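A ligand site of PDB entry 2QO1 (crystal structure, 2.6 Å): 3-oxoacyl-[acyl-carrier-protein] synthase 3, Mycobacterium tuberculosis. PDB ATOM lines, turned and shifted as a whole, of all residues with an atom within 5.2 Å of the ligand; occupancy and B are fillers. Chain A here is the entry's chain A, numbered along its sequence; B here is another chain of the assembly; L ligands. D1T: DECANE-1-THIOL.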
ATOM      1  N   ASN A  91     -25.166   2.963  -4.191  1.00  0.00           N
ATOM      2  CA  ASN A  91     -24.424   4.142  -3.771  1.00  0.00           C
ATOM      3  C   ASN A  91     -23.967   3.975  -2.324  1.00  0.00           C
ATOM      4  O   ASN A  91     -23.452   4.909  -1.711  1.00  0.00           O
ATOM      5  CB  ASN A  91     -25.273   5.402  -3.972  1.00  0.00           C
ATOM      6  CG  ASN A  91     -25.560   5.678  -5.445  1.00  0.00           C
ATOM      7  OD1 ASN A  91     -24.747   6.277  -6.155  1.00  0.00           O
ATOM      8  ND2 ASN A  91     -26.722   5.253  -5.914  1.00  0.00           N
ATOM      9  N   THR A  92     -24.134   2.761  -1.816  1.00  0.00           N
ATOM     10  CA  THR A  92     -23.928   2.438  -0.402  1.00  0.00           C
ATOM     11  C   THR A  92     -23.296   1.053  -0.168  1.00  0.00           C
ATOM     12  O   THR A  92     -23.596   0.376   0.824  1.00  0.00           O
ATOM     13  CB  THR A  92     -25.256   2.500   0.391  1.00  0.00           C
ATOM     14  OG1 THR A  92     -26.265   1.764  -0.288  1.00  0.00           O
ATOM     15  CG2 THR A  92     -25.727   3.937   0.582  1.00  0.00           C
ATOM     16  N   GLY A 121     -25.637   7.615  -8.721  1.00  0.00           N
ATOM     17  CA  GLY A 121     -26.697   8.197  -7.897  1.00  0.00           C
ATOM     18  C   GLY A 121     -27.994   7.454  -8.102  1.00  0.00           C
ATOM     19  O   GLY A 121     -28.013   6.318  -8.603  1.00  0.00           O
ATOM     20  N   CYS A 122     -29.096   8.099  -7.719  1.00  0.00           N
ATOM     21  CA  CYS A 122     -30.446   7.549  -7.859  1.00  0.00           C
ATOM     22  C   CYS A 122     -30.742   7.039  -9.277  1.00  0.00           C
ATOM     23  O   CYS A 122     -31.560   6.139  -9.464  1.00  0.00           O
ATOM     24  CB  CYS A 122     -31.472   8.618  -7.464  1.00  0.00           C
ATOM     25  SG  CYS A 122     -31.484   9.213  -5.717  1.00  0.00           S
ATOM     26  N   GLU A 150     -29.610  -0.576  -1.791  1.00  0.00           N
ATOM     27  CA  GLU A 150     -29.182   0.618  -1.088  1.00  0.00           C
ATOM     28  C   GLU A 150     -29.392   0.485   0.412  1.00  0.00           C
ATOM     29  O   GLU A 150     -30.507   0.275   0.872  1.00  0.00           O
ATOM     30  CB  GLU A 150     -29.937   1.839  -1.630  1.00  0.00           C
ATOM     31  CG  GLU A 150     -29.112   3.116  -1.742  1.00  0.00           C
ATOM     32  CD  GLU A 150     -28.179   3.132  -2.949  1.00  0.00           C
ATOM     33  OE1 GLU A 150     -27.332   2.236  -3.086  1.00  0.00           O
ATOM     34  OE2 GLU A 150     -28.280   4.073  -3.760  1.00  0.00           O
ATOM     35  N   LEU A 152     -29.102   2.971   3.168  1.00  0.00           N
ATOM     36  CA  LEU A 152     -28.908   4.409   3.379  1.00  0.00           C
ATOM     37  C   LEU A 152     -28.894   4.853   4.849  1.00  0.00           C
ATOM     38  O   LEU A 152     -28.324   5.899   5.166  1.00  0.00           O
ATOM     39  CB  LEU A 152     -29.907   5.223   2.562  1.00  0.00           C
ATOM     40  CG  LEU A 152     -29.567   5.426   1.080  1.00  0.00           C
ATOM     41  CD1 LEU A 152     -30.805   5.584   0.229  1.00  0.00           C
ATOM     42  CD2 LEU A 152     -28.618   6.607   0.872  1.00  0.00           C
ATOM     43  N   THR A 155     -25.935   6.400   6.847  1.00  0.00           N
ATOM     44  CA  THR A 155     -25.396   7.633   6.260  1.00  0.00           C
ATOM     45  C   THR A 155     -26.234   8.849   6.644  1.00  0.00           C
ATOM     46  O   THR A 155     -25.902   9.988   6.290  1.00  0.00           O
ATOM     47  CB  THR A 155     -25.310   7.519   4.712  1.00  0.00           C
ATOM     48  OG1 THR A 155     -26.608   7.607   4.138  1.00  0.00           O
ATOM     49  CG2 THR A 155     -24.652   6.211   4.281  1.00  0.00           C
ATOM     50  N   PHE A 167     -34.249   9.254   3.137  1.00  0.00           N
ATOM     51  CA  PHE A 167     -33.585   8.090   2.570  1.00  0.00           C
ATOM     52  C   PHE A 167     -33.885   6.808   3.339  1.00  0.00           C
ATOM     53  O   PHE A 167     -34.112   6.848   4.548  1.00  0.00           O
ATOM     54  CB  PHE A 167     -32.078   8.347   2.448  1.00  0.00           C
ATOM     55  CG  PHE A 167     -31.748   9.651   1.764  1.00  0.00           C
ATOM     56  CD1 PHE A 167     -31.256  10.721   2.484  1.00  0.00           C
ATOM     57  CD2 PHE A 167     -31.956   9.804   0.395  1.00  0.00           C
ATOM     58  CE1 PHE A 167     -30.958  11.931   1.851  1.00  0.00           C
ATOM     59  CE2 PHE A 167     -31.661  11.011  -0.252  1.00  0.00           C
ATOM     60  CZ  PHE A 167     -31.169  12.071   0.478  1.00  0.00           C
ATOM     61  N   ILE A 199     -26.620  16.817  -3.925  1.00  0.00           N
ATOM     62  CA  ILE A 199     -26.756  15.620  -3.097  1.00  0.00           C
ATOM     63  C   ILE A 199     -25.384  14.954  -3.042  1.00  0.00           C
ATOM     64  O   ILE A 199     -24.864  14.497  -4.066  1.00  0.00           O
ATOM     65  CB  ILE A 199     -27.789  14.620  -3.652  1.00  0.00           C
ATOM     66  CG1 ILE A 199     -29.132  15.302  -3.915  1.00  0.00           C
ATOM     67  CG2 ILE A 199     -27.950  13.430  -2.699  1.00  0.00           C
ATOM     68  CD1 ILE A 199     -30.058  14.511  -4.852  1.00  0.00           C
ATOM     69  N   ARG A 200     -24.815  14.893  -1.840  1.00  0.00           N
ATOM     70  CA  ARG A 200     -23.403  14.529  -1.682  1.00  0.00           C
ATOM     71  C   ARG A 200     -23.102  13.861  -0.342  1.00  0.00           C
ATOM     72  O   ARG A 200     -23.901  13.914   0.603  1.00  0.00           O
ATOM     73  CB  ARG A 200     -22.547  15.788  -1.803  1.00  0.00           C
ATOM     74  CG  ARG A 200     -22.582  16.659  -0.551  1.00  0.00           C
ATOM     75  CD  ARG A 200     -22.039  18.038  -0.792  1.00  0.00           C
ATOM     76  NE  ARG A 200     -21.995  18.802   0.453  1.00  0.00           N
ATOM     77  CZ  ARG A 200     -22.977  19.590   0.903  1.00  0.00           C
ATOM     78  NH1 ARG A 200     -24.094  19.740   0.202  1.00  0.00           N
ATOM     79  NH2 ARG A 200     -22.825  20.224   2.050  1.00  0.00           N
ATOM     80  N   GLN A 201     -21.938  13.224  -0.287  1.00  0.00           N
ATOM     81  CA  GLN A 201     -21.292  12.876   0.963  1.00  0.00           C
ATOM     82  C   GLN A 201     -20.466  14.105   1.319  1.00  0.00           C
ATOM     83  O   GLN A 201     -19.534  14.453   0.592  1.00  0.00           O
ATOM     84  CB  GLN A 201     -20.401  11.651   0.750  1.00  0.00           C
ATOM     85  CG  GLN A 201     -19.615  11.192   1.966  1.00  0.00           C
ATOM     86  CD  GLN A 201     -18.822   9.922   1.699  1.00  0.00           C
ATOM     87  OE1 GLN A 201     -19.284   9.037   0.984  1.00  0.00           O
ATOM     88  NE2 GLN A 201     -17.620   9.846   2.260  1.00  0.00           N
ATOM     89  N   TRP A 205     -13.962  10.125   2.310  1.00  0.00           N
ATOM     90  CA  TRP A 205     -13.497   9.063   3.199  1.00  0.00           C
ATOM     91  C   TRP A 205     -12.032   9.216   3.640  1.00  0.00           C
ATOM     92  O   TRP A 205     -11.722   9.020   4.819  1.00  0.00           O
ATOM     93  CB  TRP A 205     -13.738   7.679   2.589  1.00  0.00           C
ATOM     94  CG  TRP A 205     -15.176   7.244   2.599  1.00  0.00           C
ATOM     95  CD1 TRP A 205     -15.917   6.846   1.523  1.00  0.00           C
ATOM     96  CD2 TRP A 205     -16.054   7.143   3.744  1.00  0.00           C
ATOM     97  NE1 TRP A 205     -17.190   6.507   1.922  1.00  0.00           N
ATOM     98  CE2 TRP A 205     -17.298   6.680   3.275  1.00  0.00           C
ATOM     99  CE3 TRP A 205     -15.892   7.399   5.119  1.00  0.00           C
ATOM    100  CZ2 TRP A 205     -18.394   6.479   4.128  1.00  0.00           C
ATOM    101  CZ3 TRP A 205     -16.972   7.196   5.970  1.00  0.00           C
ATOM    102  CH2 TRP A 205     -18.215   6.740   5.468  1.00  0.00           C
ATOM    103  N   ARG A 216     -17.741  12.831  11.338  1.00  0.00           N
ATOM    104  CA  ARG A 216     -17.833  11.794  10.316  1.00  0.00           C
ATOM    105  C   ARG A 216     -18.705  12.267   9.138  1.00  0.00           C
ATOM    106  O   ARG A 216     -19.465  13.228   9.281  1.00  0.00           O
ATOM    107  CB  ARG A 216     -18.363  10.475  10.920  1.00  0.00           C
ATOM    108  CG  ARG A 216     -19.647  10.604  11.744  1.00  0.00           C
ATOM    109  CD  ARG A 216     -20.484   9.337  11.682  1.00  0.00           C
ATOM    110  NE  ARG A 216     -20.978   9.097  10.322  1.00  0.00           N
ATOM    111  CZ  ARG A 216     -21.701   8.034   9.960  1.00  0.00           C
ATOM    112  NH1 ARG A 216     -22.027   7.111  10.851  1.00  0.00           N
ATOM    113  NH2 ARG A 216     -22.107   7.912   8.704  1.00  0.00           N
ATOM    114  N   PRO A 217     -18.579  11.629   7.961  1.00  0.00           N
ATOM    115  CA  PRO A 217     -19.427  12.020   6.840  1.00  0.00           C
ATOM    116  C   PRO A 217     -20.877  11.582   7.013  1.00  0.00           C
ATOM    117  O   PRO A 217     -21.168  10.596   7.689  1.00  0.00           O
ATOM    118  CB  PRO A 217     -18.814  11.292   5.637  1.00  0.00           C
ATOM    119  CG  PRO A 217     -17.523  10.725   6.125  1.00  0.00           C
ATOM    120  CD  PRO A 217     -17.665  10.531   7.584  1.00  0.00           C
ATOM    121  N   PHE A 218     -21.773  12.338   6.387  1.00  0.00           N
ATOM    122  CA  PHE A 218     -23.180  12.015   6.326  1.00  0.00           C
ATOM    123  C   PHE A 218     -23.674  12.369   4.927  1.00  0.00           C
ATOM    124  O   PHE A 218     -22.943  13.018   4.183  1.00  0.00           O
ATOM    125  CB  PHE A 218     -23.965  12.813   7.371  1.00  0.00           C
ATOM    126  CG  PHE A 218     -23.780  12.324   8.788  1.00  0.00           C
ATOM    127  CD1 PHE A 218     -24.208  11.049   9.168  1.00  0.00           C
ATOM    128  CD2 PHE A 218     -23.227  13.156   9.757  1.00  0.00           C
ATOM    129  CE1 PHE A 218     -24.055  10.604  10.473  1.00  0.00           C
ATOM    130  CE2 PHE A 218     -23.076  12.723  11.074  1.00  0.00           C
ATOM    131  CZ  PHE A 218     -23.490  11.442  11.437  1.00  0.00           C
ATOM    132  N   VAL A 219     -24.880  11.949   4.572  1.00  0.00           N
ATOM    133  CA  VAL A 219     -25.490  12.401   3.320  1.00  0.00           C
ATOM    134  C   VAL A 219     -26.159  13.768   3.515  1.00  0.00           C
ATOM    135  O   VAL A 219     -26.932  13.951   4.445  1.00  0.00           O
ATOM    136  CB  VAL A 219     -26.490  11.364   2.709  1.00  0.00           C
ATOM    137  CG1 VAL A 219     -27.680  11.110   3.644  1.00  0.00           C
ATOM    138  CG2 VAL A 219     -26.957  11.810   1.336  1.00  0.00           C
ATOM    139  N   HIS A 258     -38.587   8.163 -10.277  1.00  0.00           N
ATOM    140  CA  HIS A 258     -37.821   7.928  -9.065  1.00  0.00           C
ATOM    141  C   HIS A 258     -38.620   8.428  -7.850  1.00  0.00           C
ATOM    142  O   HIS A 258     -39.233   9.505  -7.888  1.00  0.00           O
ATOM    143  CB  HIS A 258     -36.453   8.619  -9.124  1.00  0.00           C
ATOM    144  CG  HIS A 258     -35.645   8.427  -7.874  1.00  0.00           C
ATOM    145  ND1 HIS A 258     -35.012   7.243  -7.581  1.00  0.00           N
ATOM    146  CD2 HIS A 258     -35.392   9.267  -6.842  1.00  0.00           C
ATOM    147  CE1 HIS A 258     -34.398   7.356  -6.413  1.00  0.00           C
ATOM    148  NE2 HIS A 258     -34.606   8.575  -5.948  1.00  0.00           N
ATOM    149  N   SER A 291     -32.959   5.419  -3.556  1.00  0.00           N
ATOM    150  CA  SER A 291     -31.987   5.659  -4.636  1.00  0.00           C
ATOM    151  C   SER A 291     -32.044   4.615  -5.754  1.00  0.00           C
ATOM    152  O   SER A 291     -33.068   4.453  -6.402  1.00  0.00           O
ATOM    153  CB  SER A 291     -30.572   5.767  -4.080  1.00  0.00           C
ATOM    154  OG  SER A 291     -30.570   6.194  -2.730  1.00  0.00           O
ATOM    155  N   TYR A 319     -33.717  10.023 -11.401  1.00  0.00           N
ATOM    156  CA  TYR A 319     -33.070  11.314 -11.161  1.00  0.00           C
ATOM    157  C   TYR A 319     -32.515  11.401  -9.745  1.00  0.00           C
ATOM    158  O   TYR A 319     -33.049  10.783  -8.818  1.00  0.00           O
ATOM    159  CB  TYR A 319     -34.001  12.494 -11.470  1.00  0.00           C
ATOM    160  CG  TYR A 319     -35.305  12.533 -10.690  1.00  0.00           C
ATOM    161  CD1 TYR A 319     -35.426  13.310  -9.550  1.00  0.00           C
ATOM    162  CD2 TYR A 319     -36.416  11.805 -11.115  1.00  0.00           C
ATOM    163  CE1 TYR A 319     -36.616  13.359  -8.836  1.00  0.00           C
ATOM    164  CE2 TYR A 319     -37.616  11.845 -10.419  1.00  0.00           C
ATOM    165  CZ  TYR A 319     -37.712  12.624  -9.277  1.00  0.00           C
ATOM    166  OH  TYR A 319     -38.894  12.675  -8.580  1.00  0.00           O
ATOM    167  N   GLY A 320     -31.430  12.151  -9.578  1.00  0.00           N
ATOM    168  CA  GLY A 320     -30.794  12.336  -8.278  1.00  0.00           C
ATOM    169  C   GLY A 320     -29.338  12.750  -8.338  1.00  0.00           C
ATOM    170  O   GLY A 320     -28.929  13.498  -9.232  1.00  0.00           O
ATOM    171  N   ALA A 321     -28.562  12.215  -7.384  1.00  0.00           N
ATOM    172  CA  ALA A 321     -27.147  12.571  -7.168  1.00  0.00           C
ATOM    173  C   ALA A 321     -26.222  12.556  -8.394  1.00  0.00           C
ATOM    174  O   ALA A 321     -26.561  11.991  -9.447  1.00  0.00           O
ATOM    175  CB  ALA A 321     -26.565  11.726  -6.047  1.00  0.00           C
ATOM    176  N   GLN B  96     -19.290   8.153  -1.744  1.00  0.00           N
ATOM    177  CA  GLN B  96     -20.392   7.263  -2.106  1.00  0.00           C
ATOM    178  C   GLN B  96     -21.211   7.963  -3.184  1.00  0.00           C
ATOM    179  O   GLN B  96     -21.592   7.348  -4.174  1.00  0.00           O
ATOM    180  CB  GLN B  96     -21.277   6.949  -0.879  1.00  0.00           C
ATOM    181  CG  GLN B  96     -20.576   6.298   0.339  1.00  0.00           C
ATOM    182  CD  GLN B  96     -19.873   4.979   0.031  1.00  0.00           C
ATOM    183  OE1 GLN B  96     -18.737   4.757   0.462  1.00  0.00           O
ATOM    184  NE2 GLN B  96     -20.546   4.081  -0.702  1.00  0.00           N
ATOM    185  N   THR B  97     -21.472   9.248  -2.963  1.00  0.00           N
ATOM    186  CA  THR B  97     -22.118  10.113  -3.956  1.00  0.00           C
ATOM    187  C   THR B  97     -21.584  11.541  -3.756  1.00  0.00           C
ATOM    188  O   THR B  97     -21.207  11.904  -2.642  1.00  0.00           O
ATOM    189  CB  THR B  97     -23.685  10.053  -3.851  1.00  0.00           C
ATOM    190  OG1 THR B  97     -24.267   9.865  -5.147  1.00  0.00           O
ATOM    191  CG2 THR B  97     -24.262  11.298  -3.185  1.00  0.00           C
HETATM  192  C10 D1T L   1     -22.010   9.219   4.343  1.00  0.00           C
HETATM  193  C9  D1T L   1     -22.218   8.726   2.916  1.00  0.00           C
HETATM  194  C8  D1T L   1     -23.177   9.613   2.105  1.00  0.00           C
HETATM  195  C7  D1T L   1     -24.278   8.762   1.489  1.00  0.00           C
HETATM  196  C6  D1T L   1     -24.332   8.863  -0.034  1.00  0.00           C
HETATM  197  C5  D1T L   1     -25.436   7.992  -0.620  1.00  0.00           C
HETATM  198  C4  D1T L   1     -26.611   8.860  -1.068  1.00  0.00           C
HETATM  199  C3  D1T L   1     -27.045   8.537  -2.499  1.00  0.00           C
HETATM  200  C2  D1T L   1     -28.206   9.434  -2.958  1.00  0.00           C
HETATM  201  C1  D1T L   1     -28.649   9.005  -4.362  1.00  0.00           C
HETATM  202  S1  D1T L   1     -29.812  10.155  -5.185  1.00  0.00           S
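N of Cys 122 sits close to S1 of the ligand (3.3 Å).
A sulfur (S1) of the ligand is bonded to the side-chain sulfur (SG) of Cys 122, 2.0 Å away.
The backbone NH (N) of Ala 321 sits close to a sulfur (S1) of the ligand (3.3 Å).
The side-chain amide oxygen of Gln 201 sits at hydrogen-bond distance from the backbone NH of Gln 96 of chain B (2.9 Å).
O of Thr 97 of chain B sits at hydrogen-bond distance from N of Gln 201.
The indole nitrogen (NE1) of Trp 205 lies close to the side-chain amide nitrogen (NE2) of Gln 201 (3.4 Å).
O of Leu 152 sits at hydrogen-bond distance from OG1 of Thr 155 (2.6 Å).
The backbone carbonyl oxygen (O) of Thr 155 is in hydrogen-bond range of the backbone NH (N) of Val 219 (2.8 Å).
OE1 of Gln 96 of chain B is in hydrogen-bond range of NE1 of Trp 205 (2.8 Å).
The side-chain hydroxyl (OG) of Ser 291 lies close to the side-chain carboxylate (OE2) of Glu 150 (3.3 Å).
OD1 of Asn 91 sits at hydrogen-bond distance from N of Gly 121.
Residues that only touch the ligand: Gln 201, Leu 152, Thr 155, Phe 218, Val 219, Gln 96 of chain B, Pro 217, Ser 291, Asn 91, Gly 320 and Thr 97 of chain B.
Hydrophobic or aromatic side chains that line the ligand: Leu 152, Val 219 and Ala 321.
Within 4 Å of the ligand: Asn 91, Cys 122, Leu 152, Thr 155, Gln 201, Pro 217, Phe 218, Val 219, Ser 291, Gly 320, Ala 321, Gln 96 of chain B and Thr 97 of chain B.
The nearest printed residue that does not touch the ligand is Ile 199 (4.01 Å).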
